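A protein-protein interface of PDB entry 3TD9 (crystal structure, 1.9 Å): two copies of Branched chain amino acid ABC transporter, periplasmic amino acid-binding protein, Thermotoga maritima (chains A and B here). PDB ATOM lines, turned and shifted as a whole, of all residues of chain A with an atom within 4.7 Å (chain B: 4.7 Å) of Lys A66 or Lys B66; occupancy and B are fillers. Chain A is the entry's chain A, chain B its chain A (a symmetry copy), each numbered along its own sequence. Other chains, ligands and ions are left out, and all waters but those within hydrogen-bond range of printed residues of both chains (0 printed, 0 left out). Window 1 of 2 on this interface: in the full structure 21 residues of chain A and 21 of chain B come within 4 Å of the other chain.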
ATOM      1  N   SER A  64      14.268 -12.835 -15.914  1.00  0.00           N
ATOM      2  CA  SER A  64      14.164 -13.336 -17.283  1.00  0.00           C
ATOM      3  C   SER A  64      15.442 -14.063 -17.749  1.00  0.00           C
ATOM      4  O   SER A  64      15.734 -14.075 -18.940  1.00  0.00           O
ATOM      5  CB  SER A  64      13.816 -12.186 -18.271  1.00  0.00           C
ATOM      6  OG  SER A  64      12.578 -11.566 -17.926  1.00  0.00           O
ATOM      7  N   GLU A  65      16.172 -14.683 -16.813  1.00  0.00           N
ATOM      8  CA  GLU A  65      17.421 -15.382 -17.115  1.00  0.00           C
ATOM      9  C   GLU A  65      17.361 -16.858 -16.669  1.00  0.00           C
ATOM     10  O   GLU A  65      16.839 -17.179 -15.597  1.00  0.00           O
ATOM     11  CB  GLU A  65      18.589 -14.714 -16.372  1.00  0.00           C
ATOM     12  CG  GLU A  65      18.910 -13.339 -16.901  1.00  0.00           C
ATOM     13  CD  GLU A  65      19.965 -12.627 -16.100  1.00  0.00           C
ATOM     14  OE1 GLU A  65      20.648 -13.254 -15.263  1.00  0.00           O
ATOM     15  OE2 GLU A  65      20.123 -11.413 -16.345  1.00  0.00           O
ATOM     16  N   LYS A  66      17.912 -17.738 -17.498  1.00  0.00           N
ATOM     17  CA  LYS A  66      18.032 -19.161 -17.193  1.00  0.00           C
ATOM     18  C   LYS A  66      18.870 -19.365 -15.913  1.00  0.00           C
ATOM     19  O   LYS A  66      18.477 -20.109 -15.014  1.00  0.00           O
ATOM     20  CB  LYS A  66      18.699 -19.911 -18.386  1.00  0.00           C
ATOM     21  CG  LYS A  66      17.987 -19.820 -19.781  1.00  0.00           C
ATOM     22  CD  LYS A  66      18.896 -20.357 -20.984  1.00  0.00           C
ATOM     23  CE  LYS A  66      18.346 -19.926 -22.380  1.00  0.00           C
ATOM     24  NZ  LYS A  66      18.585 -20.863 -23.571  1.00  0.00           N
ATOM     25  N   THR A  67      20.041 -18.703 -15.845  1.00  0.00           N
ATOM     26  CA  THR A  67      20.972 -18.877 -14.706  1.00  0.00           C
ATOM     27  C   THR A  67      20.295 -18.464 -13.413  1.00  0.00           C
ATOM     28  O   THR A  67      20.362 -19.160 -12.429  1.00  0.00           O
ATOM     29  CB  THR A  67      22.299 -18.055 -14.810  1.00  0.00           C
ATOM     30  OG1 THR A  67      21.977 -16.679 -15.025  1.00  0.00           O
ATOM     31  CG2 THR A  67      23.155 -18.511 -15.937  1.00  0.00           C
ATOM     32  N   GLU A  68      19.623 -17.329 -13.427  1.00  0.00           N
ATOM     33  CA  GLU A  68      18.996 -16.825 -12.206  1.00  0.00           C
ATOM     34  C   GLU A  68      17.712 -17.580 -11.804  1.00  0.00           C
ATOM     35  O   GLU A  68      17.419 -17.687 -10.625  1.00  0.00           O
ATOM     36  CB  GLU A  68      18.748 -15.315 -12.324  1.00  0.00           C
ATOM     37  CG  GLU A  68      18.469 -14.647 -10.994  1.00  0.00           C
ATOM     38  CD  GLU A  68      19.586 -14.873  -9.955  1.00  0.00           C
ATOM     39  OE1 GLU A  68      20.782 -15.004 -10.314  1.00  0.00           O
ATOM     40  OE2 GLU A  68      19.233 -14.936  -8.765  1.00  0.00           O
ATOM     41  N   ALA A  69      16.979 -18.133 -12.773  1.00  0.00           N
ATOM     42  CA  ALA A  69      15.866 -19.024 -12.465  1.00  0.00           C
ATOM     43  C   ALA A  69      16.423 -20.214 -11.709  1.00  0.00           C
ATOM     44  O   ALA A  69      15.887 -20.613 -10.672  1.00  0.00           O
ATOM     45  CB  ALA A  69      15.154 -19.500 -13.744  1.00  0.00           C
ATOM     46  N   ALA A  70      17.512 -20.786 -12.237  1.00  0.00           N
ATOM     47  CA  ALA A  70      18.128 -21.963 -11.640  1.00  0.00           C
ATOM     48  C   ALA A  70      18.617 -21.605 -10.251  1.00  0.00           C
ATOM     49  O   ALA A  70      18.380 -22.347  -9.318  1.00  0.00           O
ATOM     50  CB  ALA A  70      19.342 -22.485 -12.509  1.00  0.00           C
ATOM     51  N   ALA A  92      11.833 -22.583 -20.998  1.00  0.00           N
ATOM     52  CA  ALA A  92      13.265 -22.661 -20.711  1.00  0.00           C
ATOM     53  C   ALA A  92      13.545 -22.489 -19.222  1.00  0.00           C
ATOM     54  O   ALA A  92      14.380 -23.196 -18.675  1.00  0.00           O
ATOM     55  CB  ALA A  92      14.065 -21.645 -21.522  1.00  0.00           C
ATOM     56  N   HIS A  93      12.868 -21.545 -18.572  1.00  0.00           N
ATOM     57  CA  HIS A  93      13.140 -21.259 -17.152  1.00  0.00           C
ATOM     58  C   HIS A  93      12.529 -22.355 -16.254  1.00  0.00           C
ATOM     59  O   HIS A  93      13.158 -22.781 -15.290  1.00  0.00           O
ATOM     60  CB  HIS A  93      12.662 -19.848 -16.792  1.00  0.00           C
ATOM     61  CG  HIS A  93      13.265 -18.791 -17.662  1.00  0.00           C
ATOM     62  ND1 HIS A  93      12.874 -17.473 -17.628  1.00  0.00           N
ATOM     63  CD2 HIS A  93      14.245 -18.870 -18.599  1.00  0.00           C
ATOM     64  CE1 HIS A  93      13.559 -16.793 -18.537  1.00  0.00           C
ATOM     65  NE2 HIS A  93      14.398 -17.622 -19.142  1.00  0.00           N
ATOM     66  N   ALA A  96      14.794 -25.252 -16.352  1.00  0.00           N
ATOM     67  CA  ALA A  96      15.994 -25.066 -15.531  1.00  0.00           C
ATOM     68  C   ALA A  96      15.692 -25.480 -14.110  1.00  0.00           C
ATOM     69  O   ALA A  96      16.545 -26.077 -13.419  1.00  0.00           O
ATOM     70  CB  ALA A  96      16.462 -23.624 -15.572  1.00  0.00           C
ATOM     71  N   VAL A 158      15.742 -19.651 -31.304  1.00  0.00           N
ATOM     72  CA  VAL A 158      16.602 -20.819 -31.004  1.00  0.00           C
ATOM     73  C   VAL A 158      17.037 -20.898 -29.543  1.00  0.00           C
ATOM     74  O   VAL A 158      17.508 -21.949 -29.073  1.00  0.00           O
ATOM     75  CB  VAL A 158      17.863 -20.860 -31.897  1.00  0.00           C
ATOM     76  CG1 VAL A 158      17.457 -20.849 -33.388  1.00  0.00           C
ATOM     77  CG2 VAL A 158      18.806 -19.720 -31.549  1.00  0.00           C
ATOM     78  N   GLU A 159      16.902 -19.789 -28.838  1.00  0.00           N
ATOM     79  CA  GLU A 159      17.312 -19.733 -27.439  1.00  0.00           C
ATOM     80  C   GLU A 159      16.218 -20.214 -26.487  1.00  0.00           C
ATOM     81  O   GLU A 159      16.464 -20.298 -25.295  1.00  0.00           O
ATOM     82  CB  GLU A 159      17.702 -18.307 -27.046  1.00  0.00           C
ATOM     83  CG  GLU A 159      18.866 -17.718 -27.862  1.00  0.00           C
ATOM     84  CD  GLU A 159      20.184 -18.503 -27.724  1.00  0.00           C
ATOM     85  OE1 GLU A 159      20.337 -19.307 -26.759  1.00  0.00           O
ATOM     86  OE2 GLU A 159      21.089 -18.304 -28.595  1.00  0.00           O
ATOM     87  N   SER B  64      29.618 -23.279 -34.371  1.00  0.00           N
ATOM     88  CA  SER B  64      29.322 -23.457 -32.950  1.00  0.00           C
ATOM     89  C   SER B  64      28.098 -22.639 -32.491  1.00  0.00           C
ATOM     90  O   SER B  64      28.024 -22.256 -31.328  1.00  0.00           O
ATOM     91  CB  SER B  64      30.559 -23.099 -32.076  1.00  0.00           C
ATOM     92  OG  SER B  64      31.678 -23.920 -32.406  1.00  0.00           O
ATOM     93  N   GLU B  65      27.141 -22.403 -33.398  1.00  0.00           N
ATOM     94  CA  GLU B  65      25.944 -21.615 -33.103  1.00  0.00           C
ATOM     95  C   GLU B  65      24.658 -22.423 -33.376  1.00  0.00           C
ATOM     96  O   GLU B  65      24.562 -23.151 -34.368  1.00  0.00           O
ATOM     97  CB  GLU B  65      25.909 -20.362 -33.991  1.00  0.00           C
ATOM     98  CG  GLU B  65      26.985 -19.365 -33.642  1.00  0.00           C
ATOM     99  CD  GLU B  65      27.040 -18.195 -34.585  1.00  0.00           C
ATOM    100  OE1 GLU B  65      26.106 -17.994 -35.389  1.00  0.00           O
ATOM    101  OE2 GLU B  65      28.037 -17.450 -34.488  1.00  0.00           O
ATOM    102  N   LYS B  66      23.678 -22.271 -32.492  1.00  0.00           N
ATOM    103  CA  LYS B  66      22.360 -22.881 -32.643  1.00  0.00           C
ATOM    104  C   LYS B  66      21.690 -22.392 -33.945  1.00  0.00           C
ATOM    105  O   LYS B  66      21.174 -23.190 -34.727  1.00  0.00           O
ATOM    106  CB  LYS B  66      21.460 -22.525 -31.420  1.00  0.00           C
ATOM    107  CG  LYS B  66      21.978 -22.946 -30.000  1.00  0.00           C
ATOM    108  CD  LYS B  66      21.148 -22.276 -28.807  1.00  0.00           C
ATOM    109  CE  LYS B  66      21.883 -22.393 -27.435  1.00  0.00           C
ATOM    110  NZ  LYS B  66      21.028 -22.499 -26.165  1.00  0.00           N
ATOM    111  N   THR B  67      21.692 -21.062 -34.163  1.00  0.00           N
ATOM    112  CA  THR B  67      21.013 -20.462 -35.334  1.00  0.00           C
ATOM    113  C   THR B  67      21.617 -20.999 -36.618  1.00  0.00           C
ATOM    114  O   THR B  67      20.913 -21.383 -37.521  1.00  0.00           O
ATOM    115  CB  THR B  67      21.091 -18.901 -35.411  1.00  0.00           C
ATOM    116  OG1 THR B  67      22.460 -18.500 -35.330  1.00  0.00           O
ATOM    117  CG2 THR B  67      20.351 -18.247 -34.299  1.00  0.00           C
ATOM    118  N   GLU B  68      22.934 -21.041 -36.687  1.00  0.00           N
ATOM    119  CA  GLU B  68      23.597 -21.482 -37.913  1.00  0.00           C
ATOM    120  C   GLU B  68      23.538 -23.006 -38.143  1.00  0.00           C
ATOM    121  O   GLU B  68      23.509 -23.444 -39.280  1.00  0.00           O
ATOM    122  CB  GLU B  68      25.042 -20.963 -37.948  1.00  0.00           C
ATOM    123  CG  GLU B  68      25.672 -21.036 -39.323  1.00  0.00           C
ATOM    124  CD  GLU B  68      24.862 -20.286 -40.402  1.00  0.00           C
ATOM    125  OE1 GLU B  68      24.190 -19.267 -40.110  1.00  0.00           O
ATOM    126  OE2 GLU B  68      24.902 -20.757 -41.551  1.00  0.00           O
ATOM    127  N   ALA B  69      23.477 -23.801 -37.071  1.00  0.00           N
ATOM    128  CA  ALA B  69      23.222 -25.231 -37.204  1.00  0.00           C
ATOM    129  C   ALA B  69      21.864 -25.399 -37.857  1.00  0.00           C
ATOM    130  O   ALA B  69      21.709 -26.173 -38.805  1.00  0.00           O
ATOM    131  CB  ALA B  69      23.237 -25.936 -35.835  1.00  0.00           C
ATOM    132  N   ALA B  70      20.871 -24.664 -37.341  1.00  0.00           N
ATOM    133  CA  ALA B  70      19.507 -24.758 -37.842  1.00  0.00           C
ATOM    134  C   ALA B  70      19.489 -24.316 -39.292  1.00  0.00           C
ATOM    135  O   ALA B  70      18.896 -24.982 -40.118  1.00  0.00           O
ATOM    136  CB  ALA B  70      18.518 -23.852 -37.003  1.00  0.00           C
ATOM    137  N   ALA B  92      22.645 -29.491 -28.079  1.00  0.00           N
ATOM    138  CA  ALA B  92      21.862 -28.313 -28.450  1.00  0.00           C
ATOM    139  C   ALA B  92      21.777 -28.153 -29.964  1.00  0.00           C
ATOM    140  O   ALA B  92      20.719 -27.826 -30.482  1.00  0.00           O
ATOM    141  CB  ALA B  92      22.411 -27.041 -27.811  1.00  0.00           C
ATOM    142  N   HIS B  93      22.887 -28.365 -30.669  1.00  0.00           N
ATOM    143  CA  HIS B  93      22.909 -28.150 -32.127  1.00  0.00           C
ATOM    144  C   HIS B  93      22.192 -29.307 -32.854  1.00  0.00           C
ATOM    145  O   HIS B  93      21.452 -29.070 -33.804  1.00  0.00           O
ATOM    146  CB  HIS B  93      24.348 -27.932 -32.610  1.00  0.00           C
ATOM    147  CG  HIS B  93      25.032 -26.805 -31.906  1.00  0.00           C
ATOM    148  ND1 HIS B  93      26.369 -26.519 -32.061  1.00  0.00           N
ATOM    149  CD2 HIS B  93      24.549 -25.884 -31.032  1.00  0.00           C
ATOM    150  CE1 HIS B  93      26.688 -25.495 -31.281  1.00  0.00           C
ATOM    151  NE2 HIS B  93      25.597 -25.093 -30.643  1.00  0.00           N
ATOM    152  N   ALA B  96      18.573 -28.707 -32.582  1.00  0.00           N
ATOM    153  CA  ALA B  96      18.098 -27.665 -33.497  1.00  0.00           C
ATOM    154  C   ALA B  96      17.791 -28.285 -34.839  1.00  0.00           C
ATOM    155  O   ALA B  96      16.810 -27.905 -35.514  1.00  0.00           O
ATOM    156  CB  ALA B  96      19.129 -26.563 -33.648  1.00  0.00           C
ATOM    157  N   VAL B 158      23.977 -23.532 -18.445  1.00  0.00           N
ATOM    158  CA  VAL B 158      22.521 -23.375 -18.669  1.00  0.00           C
ATOM    159  C   VAL B 158      22.145 -23.197 -20.138  1.00  0.00           C
ATOM    160  O   VAL B 158      20.969 -23.342 -20.518  1.00  0.00           O
ATOM    161  CB  VAL B 158      21.931 -22.196 -17.862  1.00  0.00           C
ATOM    162  CG1 VAL B 158      22.237 -22.378 -16.359  1.00  0.00           C
ATOM    163  CG2 VAL B 158      22.442 -20.869 -18.397  1.00  0.00           C
ATOM    164  N   GLU B 159      23.130 -22.863 -20.952  1.00  0.00           N
ATOM    165  CA  GLU B 159      22.887 -22.636 -22.372  1.00  0.00           C
ATOM    166  C   GLU B 159      22.937 -23.925 -23.190  1.00  0.00           C
ATOM    167  O   GLU B 159      22.666 -23.884 -24.380  1.00  0.00           O
ATOM    168  CB  GLU B 159      23.914 -21.658 -22.948  1.00  0.00           C
ATOM    169  CG  GLU B 159      23.915 -20.272 -22.281  1.00  0.00           C
ATOM    170  CD  GLU B 159      22.581 -19.514 -22.417  1.00  0.00           C
ATOM    171  OE1 GLU B 159      21.742 -19.873 -23.294  1.00  0.00           O
ATOM    172  OE2 GLU B 159      22.371 -18.533 -21.635  1.00  0.00           O
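The side-chain amino group (NZ) of Lys A66 is in salt-bridge range of the side-chain carboxylate (OE1) of Glu B159 (3.3 Å). NZ of Lys B66 is in salt-bridge range of OE1 of Glu A159 (3.3 Å).
The side-chain amino group (NZ) of Lys A66 lies within salt-bridge range of the side-chain carboxylate (OE1) of Glu A159 (3.96 Å). The side-chain amino group (NZ) of Lys B66 lies within salt-bridge range of the side-chain carboxylate (OE1) of Glu B159 (3.96 Å).
Among the printed residues, pairs that only touch across the chains: Val A158 with Thr B67 (3.5 Å), Thr A67 with Val B158 (3.5 Å), Lys A66 with Val B158 (3.7 Å), Val A158 with Lys B66 (3.7 Å), Glu A159 with Glu B159 (3.8 Å) and Lys A66 with Lys B66 (3.9 Å).
Printed residues of chain B within 4 Å of Lys A66: Lys B66 (3.9 Å), Val B158 (3.7 Å) and Glu B159 (3.3 Å). Printed residues of chain B within 4 Å of Glu A159: Lys B66 and Glu B159. Of the printed residues of chain A, Glu B159 touches Lys A66 and Glu A159. Printed residues of chain A within 4 Å of Val B158: Lys A66 and Thr A67. Ala B92 touches none of the printed residues of chain A. The nearest printed residue of chain B that does not touch Lys A66 is Ala B92 (8.4 Å). The nearest printed residue of chain A that does not touch Lys B66 is Ala A92 (8.4 Å). The nearest printed residue of chain A that does not touch Thr B67 is Glu A159 (5.8 Å).
Of the 12 printed residues of chain B, 4 touch a printed residue of chain A. Along chain B the printed residues that touch a printed residue of chain A span positions 66 to 159. Of the 12 printed residues of chain A, 4 touch a printed residue of chain B. Hydrophobic or aromatic side chains of chain A within 4 Å of the printed part of chain B: Val A158. Along chain A the printed residues that touch a printed residue of chain B span positions 66 to 159. Among the printed residues, 8 pairs touch across the chains. Among the printed residues, Asp or Glu carboxylates within 4 Å of a Lys or Arg side-chain nitrogen of the other chain: Lys A66 with Glu B159 (3.3 Å) and Glu A159 with Lys B66 (3.3 Å).
Lys B66 touches its own counterpart, Lys A66. Lys A66 touches Val B158, and with the chains exchanged Val A158 touches Lys B66. Thr A67 touches Val B158, and with the chains exchanged Val A158 touches Thr B67. Glu A159 touches its own counterpart, Glu B159. Of the 8 pairs that touch across the chains among the printed residues, 8 have their exchanged pair printed and touching as well.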
